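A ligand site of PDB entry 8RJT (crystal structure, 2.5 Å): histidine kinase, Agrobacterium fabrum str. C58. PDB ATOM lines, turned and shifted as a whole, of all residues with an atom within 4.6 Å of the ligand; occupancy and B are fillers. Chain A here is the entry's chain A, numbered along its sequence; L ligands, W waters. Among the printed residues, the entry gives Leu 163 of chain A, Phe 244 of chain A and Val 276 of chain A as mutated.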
ATOM      1  N   LEU A  10      -0.574  -6.636  -9.466  1.00  0.00           N
ATOM      2  CA  LEU A  10      -0.383  -7.109  -8.068  1.00  0.00           C
ATOM      3  C   LEU A  10       0.071  -5.948  -7.163  1.00  0.00           C
ATOM      4  O   LEU A  10       1.248  -5.938  -6.751  1.00  0.00           O
ATOM      5  CB  LEU A  10       0.594  -8.296  -8.017  1.00  0.00           C
ATOM      6  CG  LEU A  10       1.695  -8.355  -9.076  1.00  0.00           C
ATOM      7  CD1 LEU A  10       2.707  -7.238  -8.898  1.00  0.00           C
ATOM      8  CD2 LEU A  10       2.401  -9.709  -9.036  1.00  0.00           C
ATOM      9  N   CYS A  13      -4.430  -5.709  -3.710  1.00  0.00           N
ATOM     10  CA  CYS A  13      -4.819  -7.137  -3.961  1.00  0.00           C
ATOM     11  C   CYS A  13      -6.318  -7.368  -3.711  1.00  0.00           C
ATOM     12  O   CYS A  13      -6.895  -8.217  -4.417  1.00  0.00           O
ATOM     13  CB  CYS A  13      -4.017  -8.091  -3.086  1.00  0.00           C
ATOM     14  SG  CYS A  13      -2.482  -8.668  -3.858  1.00  0.00           S
ATOM     15  N   GLU A  16      -9.709  -7.066  -6.909  1.00  0.00           N
ATOM     16  CA  GLU A  16     -10.186  -7.947  -8.016  1.00  0.00           C
ATOM     17  C   GLU A  16     -11.545  -8.564  -7.664  1.00  0.00           C
ATOM     18  O   GLU A  16     -11.693  -9.147  -6.596  1.00  0.00           O
ATOM     19  CB  GLU A  16      -9.172  -9.062  -8.289  1.00  0.00           C
ATOM     20  CG  GLU A  16      -9.529  -9.952  -9.471  1.00  0.00           C
ATOM     21  CD  GLU A  16      -8.679 -11.200  -9.634  1.00  0.00           C
ATOM     22  OE1 GLU A  16      -7.694 -11.355  -8.872  1.00  0.00           O
ATOM     23  OE2 GLU A  16      -8.994 -12.017 -10.518  1.00  0.00           O
ATOM     24  N   ILE A  18     -13.482 -11.476  -7.973  1.00  0.00           N
ATOM     25  CA  ILE A  18     -13.251 -12.913  -8.325  1.00  0.00           C
ATOM     26  C   ILE A  18     -14.591 -13.651  -8.457  1.00  0.00           C
ATOM     27  O   ILE A  18     -14.583 -14.769  -8.998  1.00  0.00           O
ATOM     28  CB  ILE A  18     -12.325 -13.602  -7.307  1.00  0.00           C
ATOM     29  CG1 ILE A  18     -12.851 -13.507  -5.871  1.00  0.00           C
ATOM     30  CG2 ILE A  18     -10.912 -13.048  -7.425  1.00  0.00           C
ATOM     31  CD1 ILE A  18     -12.131 -14.400  -4.886  1.00  0.00           C
ATOM     32  N   LEU A 163      -2.176 -29.654   3.108  1.00  0.00           N
ATOM     33  CA  LEU A 163      -1.788 -28.656   4.148  1.00  0.00           C
ATOM     34  C   LEU A 163      -3.000 -28.304   5.006  1.00  0.00           C
ATOM     35  O   LEU A 163      -4.147 -28.386   4.490  1.00  0.00           O
ATOM     36  CB  LEU A 163      -1.256 -27.394   3.473  1.00  0.00           C
ATOM     37  CG  LEU A 163      -0.058 -27.569   2.546  1.00  0.00           C
ATOM     38  CD1 LEU A 163       0.343 -26.227   1.941  1.00  0.00           C
ATOM     39  CD2 LEU A 163       1.111 -28.188   3.290  1.00  0.00           C
ATOM     40  N   PHE A 187       6.390 -27.061   3.319  1.00  0.00           N
ATOM     41  CA  PHE A 187       5.996 -25.687   3.703  1.00  0.00           C
ATOM     42  C   PHE A 187       5.669 -25.617   5.199  1.00  0.00           C
ATOM     43  O   PHE A 187       5.213 -24.551   5.663  1.00  0.00           O
ATOM     44  CB  PHE A 187       4.811 -25.216   2.857  1.00  0.00           C
ATOM     45  CG  PHE A 187       5.082 -25.163   1.375  1.00  0.00           C
ATOM     46  CD1 PHE A 187       6.143 -24.424   0.877  1.00  0.00           C
ATOM     47  CD2 PHE A 187       4.264 -25.833   0.473  1.00  0.00           C
ATOM     48  CE1 PHE A 187       6.389 -24.365  -0.487  1.00  0.00           C
ATOM     49  CE2 PHE A 187       4.510 -25.774  -0.890  1.00  0.00           C
ATOM     50  CZ  PHE A 187       5.569 -25.043  -1.365  1.00  0.00           C
ATOM     51  N   PHE A 192       2.805 -16.920   5.479  1.00  0.00           N
ATOM     52  CA  PHE A 192       2.467 -16.227   4.204  1.00  0.00           C
ATOM     53  C   PHE A 192       1.682 -14.959   4.520  1.00  0.00           C
ATOM     54  O   PHE A 192       0.879 -14.944   5.441  1.00  0.00           O
ATOM     55  CB  PHE A 192       1.765 -17.214   3.267  1.00  0.00           C
ATOM     56  CG  PHE A 192       2.610 -18.425   2.986  1.00  0.00           C
ATOM     57  CD1 PHE A 192       3.700 -18.344   2.146  1.00  0.00           C
ATOM     58  CD2 PHE A 192       2.372 -19.632   3.635  1.00  0.00           C
ATOM     59  CE1 PHE A 192       4.512 -19.442   1.907  1.00  0.00           C
ATOM     60  CE2 PHE A 192       3.186 -20.737   3.401  1.00  0.00           C
ATOM     61  CZ  PHE A 192       4.248 -20.639   2.544  1.00  0.00           C
ATOM     62  N   SER A 195      -2.089 -10.618   2.342  1.00  0.00           N
ATOM     63  CA  SER A 195      -2.363 -10.203   0.934  1.00  0.00           C
ATOM     64  C   SER A 195      -2.459 -11.420   0.002  1.00  0.00           C
ATOM     65  O   SER A 195      -3.197 -11.320  -0.994  1.00  0.00           O
ATOM     66  CB  SER A 195      -1.330  -9.222   0.457  1.00  0.00           C
ATOM     67  OG  SER A 195      -0.051  -9.834   0.361  1.00  0.00           O
ATOM     68  N   ASP A 196      -1.756 -12.518   0.325  1.00  0.00           N
ATOM     69  CA  ASP A 196      -1.713 -13.758  -0.506  1.00  0.00           C
ATOM     70  C   ASP A 196      -3.087 -14.428  -0.570  1.00  0.00           C
ATOM     71  O   ASP A 196      -3.295 -15.248  -1.484  1.00  0.00           O
ATOM     72  CB  ASP A 196      -0.645 -14.736  -0.002  1.00  0.00           C
ATOM     73  CG  ASP A 196       0.772 -14.380  -0.427  1.00  0.00           C
ATOM     74  OD1 ASP A 196       1.038 -13.186  -0.650  1.00  0.00           O
ATOM     75  OD2 ASP A 196       1.598 -15.305  -0.517  1.00  0.00           O
ATOM     76  N   ILE A 197      -3.979 -14.132   0.378  1.00  0.00           N
ATOM     77  CA  ILE A 197      -5.433 -14.505   0.309  1.00  0.00           C
ATOM     78  C   ILE A 197      -6.234 -13.250   0.614  1.00  0.00           C
ATOM     79  O   ILE A 197      -6.559 -12.961   1.769  1.00  0.00           O
ATOM     80  CB  ILE A 197      -5.776 -15.691   1.244  1.00  0.00           C
ATOM     81  CG1 ILE A 197      -4.896 -16.912   0.970  1.00  0.00           C
ATOM     82  CG2 ILE A 197      -7.262 -16.040   1.152  1.00  0.00           C
ATOM     83  CD1 ILE A 197      -5.147 -18.081   1.891  1.00  0.00           C
ATOM     84  N   PRO A 198      -6.580 -12.446  -0.430  1.00  0.00           N
ATOM     85  CA  PRO A 198      -7.322 -11.199  -0.243  1.00  0.00           C
ATOM     86  C   PRO A 198      -8.654 -11.323   0.518  1.00  0.00           C
ATOM     87  O   PRO A 198      -9.103 -12.428   0.742  1.00  0.00           O
ATOM     88  CB  PRO A 198      -7.606 -10.732  -1.679  1.00  0.00           C
ATOM     89  CG  PRO A 198      -6.530 -11.388  -2.526  1.00  0.00           C
ATOM     90  CD  PRO A 198      -6.265 -12.714  -1.840  1.00  0.00           C
ATOM     91  N   GLN A 200     -11.879 -10.321  -0.226  1.00  0.00           N
ATOM     92  CA  GLN A 200     -13.060 -10.784  -1.023  1.00  0.00           C
ATOM     93  C   GLN A 200     -12.980 -12.304  -1.188  1.00  0.00           C
ATOM     94  O   GLN A 200     -14.044 -12.937  -1.342  1.00  0.00           O
ATOM     95  CB  GLN A 200     -13.151 -10.038  -2.358  1.00  0.00           C
ATOM     96  CG  GLN A 200     -12.105 -10.422  -3.396  1.00  0.00           C
ATOM     97  CD  GLN A 200     -10.767  -9.768  -3.187  1.00  0.00           C
ATOM     98  OE1 GLN A 200     -10.483  -9.191  -2.130  1.00  0.00           O
ATOM     99  NE2 GLN A 200      -9.902  -9.853  -4.188  1.00  0.00           N
ATOM    100  N   ALA A 201     -11.767 -12.874  -1.136  1.00  0.00           N
ATOM    101  CA  ALA A 201     -11.524 -14.328  -1.179  1.00  0.00           C
ATOM    102  C   ALA A 201     -12.027 -14.976   0.110  1.00  0.00           C
ATOM    103  O   ALA A 201     -12.806 -15.945   0.033  1.00  0.00           O
ATOM    104  CB  ALA A 201     -10.056 -14.614  -1.414  1.00  0.00           C
ATOM    105  N   TYR A 205     -15.032 -17.726   0.880  1.00  0.00           N
ATOM    106  CA  TYR A 205     -14.648 -19.000   1.537  1.00  0.00           C
ATOM    107  C   TYR A 205     -15.514 -19.218   2.784  1.00  0.00           C
ATOM    108  O   TYR A 205     -15.640 -20.367   3.230  1.00  0.00           O
ATOM    109  CB  TYR A 205     -13.151 -19.023   1.833  1.00  0.00           C
ATOM    110  CG  TYR A 205     -12.259 -18.845   0.624  1.00  0.00           C
ATOM    111  CD1 TYR A 205     -12.786 -18.814  -0.661  1.00  0.00           C
ATOM    112  CD2 TYR A 205     -10.892 -18.719   0.760  1.00  0.00           C
ATOM    113  CE1 TYR A 205     -11.982 -18.638  -1.771  1.00  0.00           C
ATOM    114  CE2 TYR A 205     -10.062 -18.553  -0.339  1.00  0.00           C
ATOM    115  CZ  TYR A 205     -10.613 -18.515  -1.606  1.00  0.00           C
ATOM    116  OH  TYR A 205      -9.820 -18.367  -2.714  1.00  0.00           O
ATOM    117  N   ARG A 211     -13.980 -25.756  -2.490  1.00  0.00           N
ATOM    118  CA  ARG A 211     -13.527 -25.127  -3.767  1.00  0.00           C
ATOM    119  C   ARG A 211     -12.599 -26.095  -4.506  1.00  0.00           C
ATOM    120  O   ARG A 211     -11.806 -26.771  -3.824  1.00  0.00           O
ATOM    121  CB  ARG A 211     -12.796 -23.814  -3.496  1.00  0.00           C
ATOM    122  CG  ARG A 211     -13.712 -22.670  -3.122  1.00  0.00           C
ATOM    123  CD  ARG A 211     -12.954 -21.507  -2.499  1.00  0.00           C
ATOM    124  NE  ARG A 211     -12.063 -21.906  -1.429  1.00  0.00           N
ATOM    125  CZ  ARG A 211     -12.438 -22.315  -0.216  1.00  0.00           C
ATOM    126  NH1 ARG A 211     -11.525 -22.652   0.673  1.00  0.00           N
ATOM    127  NH2 ARG A 211     -13.722 -22.394   0.096  1.00  0.00           N
ATOM    128  N   ILE A 213     -10.059 -26.505  -8.209  1.00  0.00           N
ATOM    129  CA  ILE A 213      -9.423 -26.183  -9.519  1.00  0.00           C
ATOM    130  C   ILE A 213      -9.006 -27.510 -10.155  1.00  0.00           C
ATOM    131  O   ILE A 213      -8.094 -28.163  -9.605  1.00  0.00           O
ATOM    132  CB  ILE A 213      -8.258 -25.187  -9.356  1.00  0.00           C
ATOM    133  CG1 ILE A 213      -8.670 -23.958  -8.547  1.00  0.00           C
ATOM    134  CG2 ILE A 213      -7.686 -24.807 -10.717  1.00  0.00           C
ATOM    135  CD1 ILE A 213      -7.519 -23.050  -8.156  1.00  0.00           C
ATOM    136  N   ARG A 242     -17.150 -21.867 -11.202  1.00  0.00           N
ATOM    137  CA  ARG A 242     -16.511 -20.513 -11.227  1.00  0.00           C
ATOM    138  C   ARG A 242     -15.000 -20.652 -11.473  1.00  0.00           C
ATOM    139  O   ARG A 242     -14.356 -21.421 -10.753  1.00  0.00           O
ATOM    140  CB  ARG A 242     -16.762 -19.787  -9.905  1.00  0.00           C
ATOM    141  CG  ARG A 242     -16.171 -18.396  -9.813  1.00  0.00           C
ATOM    142  CD  ARG A 242     -16.334 -17.779  -8.431  1.00  0.00           C
ATOM    143  NE  ARG A 242     -15.679 -18.580  -7.402  1.00  0.00           N
ATOM    144  CZ  ARG A 242     -14.425 -18.447  -6.995  1.00  0.00           C
ATOM    145  NH1 ARG A 242     -13.939 -19.251  -6.056  1.00  0.00           N
ATOM    146  NH2 ARG A 242     -13.629 -17.519  -7.515  1.00  0.00           N
ATOM    147  N   PHE A 244     -11.099 -19.355 -11.345  1.00  0.00           N
ATOM    148  CA  PHE A 244     -10.320 -18.682 -10.256  1.00  0.00           C
ATOM    149  C   PHE A 244      -9.447 -17.575 -10.861  1.00  0.00           C
ATOM    150  O   PHE A 244      -9.162 -17.622 -12.074  1.00  0.00           O
ATOM    151  CB  PHE A 244      -9.502 -19.709  -9.466  1.00  0.00           C
ATOM    152  CG  PHE A 244     -10.276 -20.486  -8.422  1.00  0.00           C
ATOM    153  CD1 PHE A 244     -11.483 -21.091  -8.736  1.00  0.00           C
ATOM    154  CD2 PHE A 244      -9.784 -20.628  -7.133  1.00  0.00           C
ATOM    155  CE1 PHE A 244     -12.187 -21.815  -7.786  1.00  0.00           C
ATOM    156  CE2 PHE A 244     -10.488 -21.353  -6.184  1.00  0.00           C
ATOM    157  CZ  PHE A 244     -11.687 -21.936  -6.506  1.00  0.00           C
ATOM    158  N   SER A 245      -9.066 -16.603 -10.036  1.00  0.00           N
ATOM    159  CA  SER A 245      -8.160 -15.479 -10.414  1.00  0.00           C
ATOM    160  C   SER A 245      -6.932 -16.012 -11.143  1.00  0.00           C
ATOM    161  O   SER A 245      -6.318 -16.985 -10.708  1.00  0.00           O
ATOM    162  CB  SER A 245      -7.745 -14.665  -9.219  1.00  0.00           C
ATOM    163  OG  SER A 245      -6.671 -13.798  -9.539  1.00  0.00           O
ATOM    164  N   ILE A 247      -4.094 -14.711 -11.134  1.00  0.00           N
ATOM    165  CA  ILE A 247      -2.958 -14.440 -10.200  1.00  0.00           C
ATOM    166  C   ILE A 247      -2.664 -15.744  -9.447  1.00  0.00           C
ATOM    167  O   ILE A 247      -1.492 -16.167  -9.424  1.00  0.00           O
ATOM    168  CB  ILE A 247      -3.268 -13.303  -9.196  1.00  0.00           C
ATOM    169  CG1 ILE A 247      -3.771 -12.019  -9.878  1.00  0.00           C
ATOM    170  CG2 ILE A 247      -2.048 -13.025  -8.320  1.00  0.00           C
ATOM    171  CD1 ILE A 247      -2.808 -11.421 -10.874  1.00  0.00           C
ATOM    172  N   HIS A 248      -3.709 -16.341  -8.872  1.00  0.00           N
ATOM    173  CA  HIS A 248      -3.613 -17.593  -8.076  1.00  0.00           C
ATOM    174  C   HIS A 248      -3.196 -18.752  -8.980  1.00  0.00           C
ATOM    175  O   HIS A 248      -2.330 -19.527  -8.554  1.00  0.00           O
ATOM    176  CB  HIS A 248      -4.930 -17.880  -7.345  1.00  0.00           C
ATOM    177  CG  HIS A 248      -4.840 -19.062  -6.440  1.00  0.00           C
ATOM    178  ND1 HIS A 248      -3.836 -19.195  -5.506  1.00  0.00           N
ATOM    179  CD2 HIS A 248      -5.611 -20.173  -6.334  1.00  0.00           C
ATOM    180  CE1 HIS A 248      -3.987 -20.342  -4.864  1.00  0.00           C
ATOM    181  NE2 HIS A 248      -5.065 -20.956  -5.357  1.00  0.00           N
ATOM    182  N   TYR A 251       0.367 -18.595  -9.742  1.00  0.00           N
ATOM    183  CA  TYR A 251       1.029 -19.010  -8.468  1.00  0.00           C
ATOM    184  C   TYR A 251       1.172 -20.533  -8.460  1.00  0.00           C
ATOM    185  O   TYR A 251       2.315 -21.030  -8.270  1.00  0.00           O
ATOM    186  CB  TYR A 251       0.223 -18.511  -7.258  1.00  0.00           C
ATOM    187  CG  TYR A 251       1.038 -18.295  -6.000  1.00  0.00           C
ATOM    188  CD1 TYR A 251       1.644 -19.362  -5.347  1.00  0.00           C
ATOM    189  CD2 TYR A 251       1.176 -17.030  -5.459  1.00  0.00           C
ATOM    190  CE1 TYR A 251       2.392 -19.169  -4.195  1.00  0.00           C
ATOM    191  CE2 TYR A 251       1.925 -16.822  -4.305  1.00  0.00           C
ATOM    192  CZ  TYR A 251       2.535 -17.889  -3.670  1.00  0.00           C
ATOM    193  OH  TYR A 251       3.263 -17.692  -2.539  1.00  0.00           O
ATOM    194  N   MET A 255       4.453 -23.170  -8.693  1.00  0.00           N
ATOM    195  CA  MET A 255       4.679 -24.175  -7.611  1.00  0.00           C
ATOM    196  C   MET A 255       4.732 -25.590  -8.202  1.00  0.00           C
ATOM    197  O   MET A 255       5.109 -26.515  -7.461  1.00  0.00           O
ATOM    198  CB  MET A 255       3.569 -24.121  -6.571  1.00  0.00           C
ATOM    199  CG  MET A 255       3.641 -22.916  -5.646  1.00  0.00           C
ATOM    200  SD  MET A 255       2.268 -22.914  -4.454  1.00  0.00           S
ATOM    201  CE  MET A 255       2.731 -24.287  -3.402  1.00  0.00           C
ATOM    202  N   SER A 260      -6.094 -28.348  -7.379  1.00  0.00           N
ATOM    203  CA  SER A 260      -6.263 -28.027  -5.940  1.00  0.00           C
ATOM    204  C   SER A 260      -7.691 -28.357  -5.491  1.00  0.00           C
ATOM    205  O   SER A 260      -8.600 -28.392  -6.343  1.00  0.00           O
ATOM    206  CB  SER A 260      -5.937 -26.570  -5.659  1.00  0.00           C
ATOM    207  OG  SER A 260      -6.992 -25.732  -6.099  1.00  0.00           O
ATOM    208  N   SER A 262      -9.726 -27.065  -1.735  1.00  0.00           N
ATOM    209  CA  SER A 262      -9.651 -26.426  -0.382  1.00  0.00           C
ATOM    210  C   SER A 262     -10.983 -26.605   0.357  1.00  0.00           C
ATOM    211  O   SER A 262     -12.039 -26.617  -0.307  1.00  0.00           O
ATOM    212  CB  SER A 262      -9.236 -24.974  -0.480  1.00  0.00           C
ATOM    213  OG  SER A 262     -10.137 -24.245  -1.289  1.00  0.00           O
ATOM    214  N   LEU A 274      -7.837 -23.076   6.356  1.00  0.00           N
ATOM    215  CA  LEU A 274      -8.170 -23.949   5.205  1.00  0.00           C
ATOM    216  C   LEU A 274      -7.445 -25.290   5.340  1.00  0.00           C
ATOM    217  O   LEU A 274      -6.275 -25.288   5.762  1.00  0.00           O
ATOM    218  CB  LEU A 274      -7.734 -23.260   3.910  1.00  0.00           C
ATOM    219  CG  LEU A 274      -8.282 -21.851   3.677  1.00  0.00           C
ATOM    220  CD1 LEU A 274      -7.593 -21.213   2.470  1.00  0.00           C
ATOM    221  CD2 LEU A 274      -9.786 -21.892   3.469  1.00  0.00           C
ATOM    222  N   VAL A 276      -6.012 -27.539   2.613  1.00  0.00           N
ATOM    223  CA  VAL A 276      -5.643 -27.255   1.189  1.00  0.00           C
ATOM    224  C   VAL A 276      -4.945 -28.482   0.591  1.00  0.00           C
ATOM    225  O   VAL A 276      -3.882 -28.863   1.096  1.00  0.00           O
ATOM    226  CB  VAL A 276      -4.748 -26.002   1.084  1.00  0.00           C
ATOM    227  CG1 VAL A 276      -4.377 -25.696  -0.361  1.00  0.00           C
ATOM    228  CG2 VAL A 276      -5.406 -24.795   1.725  1.00  0.00           C
ATOM    229  N   HIS A 278      -3.124 -30.101  -2.800  1.00  0.00           N
ATOM    230  CA  HIS A 278      -2.403 -29.864  -4.084  1.00  0.00           C
ATOM    231  C   HIS A 278      -2.196 -31.184  -4.831  1.00  0.00           C
ATOM    232  O   HIS A 278      -1.806 -32.174  -4.179  1.00  0.00           O
ATOM    233  CB  HIS A 278      -1.040 -29.214  -3.840  1.00  0.00           C
ATOM    234  CG  HIS A 278      -1.094 -27.812  -3.350  1.00  0.00           C
ATOM    235  ND1 HIS A 278      -0.027 -27.224  -2.701  1.00  0.00           N
ATOM    236  CD2 HIS A 278      -2.069 -26.882  -3.382  1.00  0.00           C
ATOM    237  CE1 HIS A 278      -0.340 -26.000  -2.374  1.00  0.00           C
ATOM    238  NE2 HIS A 278      -1.595 -25.756  -2.782  1.00  0.00           N
ATOM    239  N   ARG A 456       7.122 -12.521  -7.567  1.00  0.00           N
ATOM    240  CA  ARG A 456       6.219 -12.240  -6.415  1.00  0.00           C
ATOM    241  C   ARG A 456       5.343 -13.471  -6.138  1.00  0.00           C
ATOM    242  O   ARG A 456       5.060 -13.728  -4.949  1.00  0.00           O
ATOM    243  CB  ARG A 456       5.352 -11.009  -6.670  1.00  0.00           C
ATOM    244  CG  ARG A 456       4.249 -10.776  -5.654  1.00  0.00           C
ATOM    245  CD  ARG A 456       4.749 -10.572  -4.241  1.00  0.00           C
ATOM    246  NE  ARG A 456       3.663 -10.343  -3.286  1.00  0.00           N
ATOM    247  CZ  ARG A 456       3.027 -11.286  -2.596  1.00  0.00           C
ATOM    248  NH1 ARG A 456       3.348 -12.561  -2.723  1.00  0.00           N
ATOM    249  NH2 ARG A 456       2.052 -10.940  -1.769  1.00  0.00           N
ATOM    250  N   LEU A 457       4.932 -14.191  -7.179  1.00  0.00           N
ATOM    251  CA  LEU A 457       4.015 -15.364  -7.079  1.00  0.00           C
ATOM    252  C   LEU A 457       4.834 -16.652  -6.879  1.00  0.00           C
ATOM    253  O   LEU A 457       4.704 -17.576  -7.705  1.00  0.00           O
ATOM    254  CB  LEU A 457       3.157 -15.442  -8.344  1.00  0.00           C
ATOM    255  CG  LEU A 457       2.414 -14.153  -8.722  1.00  0.00           C
ATOM    256  CD1 LEU A 457       1.522 -14.390  -9.927  1.00  0.00           C
ATOM    257  CD2 LEU A 457       1.603 -13.608  -7.552  1.00  0.00           C
ATOM    258  N   PRO A 459       6.191 -19.192  -3.247  1.00  0.00           N
ATOM    259  CA  PRO A 459       6.358 -19.361  -1.800  1.00  0.00           C
ATOM    260  C   PRO A 459       7.637 -18.746  -1.215  1.00  0.00           C
ATOM    261  O   PRO A 459       7.615 -18.393  -0.043  1.00  0.00           O
ATOM    262  CB  PRO A 459       6.395 -20.883  -1.631  1.00  0.00           C
ATOM    263  CG  PRO A 459       5.562 -21.412  -2.782  1.00  0.00           C
ATOM    264  CD  PRO A 459       5.811 -20.439  -3.922  1.00  0.00           C
HETATM  265  C1  LIG L   1      -1.010 -13.641  -4.040  1.00  0.00           C
HETATM  266  C2  LIG L   1      -5.373 -14.334  -4.451  1.00  0.00           C
HETATM  267  O1  LIG L   1     -10.476 -16.991  -7.403  1.00  0.00           O
HETATM  268  C3  LIG L   1      -5.314 -18.329  -2.584  1.00  0.00           C
HETATM  269  O2  LIG L   1      -8.264 -23.245  -3.647  1.00  0.00           O
HETATM  270  C4  LIG L   1      -1.271 -20.212  -1.112  1.00  0.00           C
HETATM  271  C5  LIG L   1      -1.146 -12.328  -4.474  1.00  0.00           C
HETATM  272  C6  LIG L   1      -6.699 -14.392  -4.852  1.00  0.00           C
HETATM  273  O3  LIG L   1     -10.978 -17.930  -5.480  1.00  0.00           O
HETATM  274  C7  LIG L   1      -5.596 -19.526  -1.939  1.00  0.00           C
HETATM  275  O4  LIG L   1      -9.154 -21.807  -2.213  1.00  0.00           O
HETATM  276  C8  LIG L   1       0.098 -20.236  -0.885  1.00  0.00           C
HETATM  277  C9  LIG L   1      -2.448 -11.976  -4.772  1.00  0.00           C
HETATM  278  C10 LIG L   1      -7.185 -15.626  -4.478  1.00  0.00           C
HETATM  279  C11 LIG L   1      -4.465 -19.950  -1.297  1.00  0.00           C
HETATM  280  C12 LIG L   1       0.511 -21.572  -0.842  1.00  0.00           C
HETATM  281  C13 LIG L   1      -3.156 -13.145  -4.514  1.00  0.00           C
HETATM  282  C14 LIG L   1      -6.144 -16.280  -3.829  1.00  0.00           C
HETATM  283  C15 LIG L   1      -3.451 -19.011  -1.485  1.00  0.00           C
HETATM  284  C16 LIG L   1      -0.617 -22.352  -1.060  1.00  0.00           C
HETATM  285  C17 LIG L   1      -2.956 -10.730  -5.232  1.00  0.00           C
HETATM  286  C18 LIG L   1      -8.573 -16.164  -4.685  1.00  0.00           C
HETATM  287  C19 LIG L   1      -6.918 -20.246  -1.953  1.00  0.00           C
HETATM  288  C20 LIG L   1       1.764 -22.178  -0.617  1.00  0.00           C
HETATM  289  C21 LIG L   1      -2.365  -9.538  -5.230  1.00  0.00           C
HETATM  290  C22 LIG L   1      -8.732 -17.192  -5.802  1.00  0.00           C
HETATM  291  C23 LIG L   1      -6.884 -21.480  -2.857  1.00  0.00           C
HETATM  292  C24 LIG L   1       2.921 -21.612  -0.317  1.00  0.00           C
HETATM  293  C25 LIG L   1     -10.171 -17.388  -6.253  1.00  0.00           C
HETATM  294  C26 LIG L   1      -8.204 -22.232  -2.914  1.00  0.00           C
HETATM  295  C27 LIG L   1      -4.534 -13.248  -4.650  1.00  0.00           C
HETATM  296  C28 LIG L   1      -6.231 -17.564  -3.306  1.00  0.00           C
HETATM  297  C29 LIG L   1      -2.104 -19.091  -1.154  1.00  0.00           C
HETATM  298  C30 LIG L   1       0.019 -11.404  -4.588  1.00  0.00           C
HETATM  299  C31 LIG L   1      -7.468 -13.330  -5.582  1.00  0.00           C
HETATM  300  C32 LIG L   1      -4.369 -21.217  -0.502  1.00  0.00           C
HETATM  301  C33 LIG L   1       0.962 -19.017  -0.703  1.00  0.00           C
HETATM  302  N1  LIG L   1      -2.300 -14.155  -4.070  1.00  0.00           N
HETATM  303  O5  LIG L   1      -0.014 -14.225  -3.704  1.00  0.00           O
HETATM  304  N2  LIG L   1      -5.030 -15.492  -3.797  1.00  0.00           N
HETATM  305  N3  LIG L   1      -4.003 -18.028  -2.285  1.00  0.00           N
HETATM  306  N4  LIG L   1      -1.687 -21.520  -1.231  1.00  0.00           N
HETATM  307  O6  LIG L   1      -0.683 -23.569  -1.079  1.00  0.00           O
HETATM  308  O   HOH W   1      -3.873 -23.257  -2.865  1.00  0.00           O
HETATM  309  O   HOH W   2      -1.897 -17.132  -4.498  1.00  0.00           O
HETATM  310  O   HOH W   3      -5.869 -23.559  -4.664  1.00  0.00           O
HETATM  311  O   HOH W   4     -12.041 -15.734 -10.160  1.00  0.00           O
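The side-chain amide nitrogen (NE2) of Gln 200 lies within hydrogen-bond range of the backbone carbonyl oxygen (O) of Cys 13, 3.4 Å away. The side-chain hydroxyl (OG) of Ser 262 sits at hydrogen-bond distance from the guanidinium group (NH1) of Arg 211, at 2.9 Å. The side-chain carboxylate of Asp 196 lies within salt-bridge range of the guanidinium group of Arg 456 (2.7 Å). N of Ile 247 lies close to OG of Ser 245, 3.2 Å away. The guanidinium group of Arg 242 sits at hydrogen-bond distance from the backbone carbonyl oxygen of Ile 18. OG of Ser 195 is in hydrogen-bond range of NH2 of Arg 456, at 3.2 Å. The backbone carbonyl oxygen (O) of Ile 213 lies within hydrogen-bond range of the backbone NH (N) of Ser 260, at 3.0 Å. O of Glu 16 lies within hydrogen-bond range of NE2 of Gln 200.
Glu 16 touches the ligand (OE1 to C31, 3.8 Å). Ile 18 touches the ligand (CD1 to O3, 3.8 Å). CZ of Phe 192 touches C24 of the ligand (3.3 Å). Ser 195 touches the ligand. Ile 197 touches the ligand. CD of Pro 198 touches C2 of the ligand, 3.2 Å away. Ala 201 touches the ligand. Phe 244 touches the ligand (CA to O1, 3.3 Å). Ile 247 touches the ligand (CG2 to C9, 3.7 Å). Tyr 251 touches the ligand. Met 255 touches the ligand (CE to C20, 3.6 Å). OG of Ser 260 touches O2 of the ligand (3.7 Å). Arg 456 touches the ligand. Pro 459 touches the ligand. Hydrophobic or aromatic side chains that line the ligand: Ile 18, Phe 192, Ile 197, Pro 198, Ala 201, Tyr 205, Phe 244, Ile 247, His 248, Tyr 251, Met 255, His 278 and Pro 459. Within 4 Å of the ligand: Cys 13, Glu 16, Ile 18, Phe 192, Ser 195, Asp 196, Ile 197, Pro 198, Ala 201, Tyr 205, Arg 211, Arg 242, Phe 244, Ser 245, Ile 247, His 248, Tyr 251, Met 255, Ser 260, Ser 262, His 278, Arg 456 and Pro 459. The nearest printed residue that does not touch the ligand is Leu 457 (4.02 Å).
Water W3 lies within hydrogen-bond range of O2 of the ligand (2.6 Å), NE2 of His 248 (2.8 Å) and OG of Ser 260 (2.8 Å). Water W2 bridges a ring nitrogen (ND1) of His 248 (3.0 Å) and a nitrogen (N1) of the ligand (3.0 Å). Water W1 bridges a nitrogen (N4) of the ligand and a ring nitrogen (NE2) of His 278. Water W4 lies within hydrogen-bond range of O of Ile 18, N of Ser 245 and O1 of the ligand.
The side-chain sulfur (SG) of Cys 13 is bonded to a carbon (C21) of the ligand (1.6 Å). A ring nitrogen (NE2) of His 278 lies close to an oxygen (O6) of the ligand (2.9 Å). The side-chain hydroxyl (OG) of Ser 262 lies within hydrogen-bond range of an oxygen (O4) of the ligand, at 2.8 Å. O of Asp 196 lies within hydrogen-bond range of N3 of the ligand. N of Ser 245 lies within hydrogen-bond range of O1 of the ligand, 3.0 Å away. O4 of the ligand lies within salt-bridge range of NE of Arg 211 (3.0 Å). The side-chain hydroxyl of Tyr 205 lies within hydrogen-bond range of an oxygen (O3) of the ligand, 3.0 Å away. A ring nitrogen (ND1) of His 248 sits close to a nitrogen (N3) of the ligand (3.4 Å). The guanidinium group (NH2) of Arg 242 is in salt-bridge range of an oxygen (O1) of the ligand (3.2 Å).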
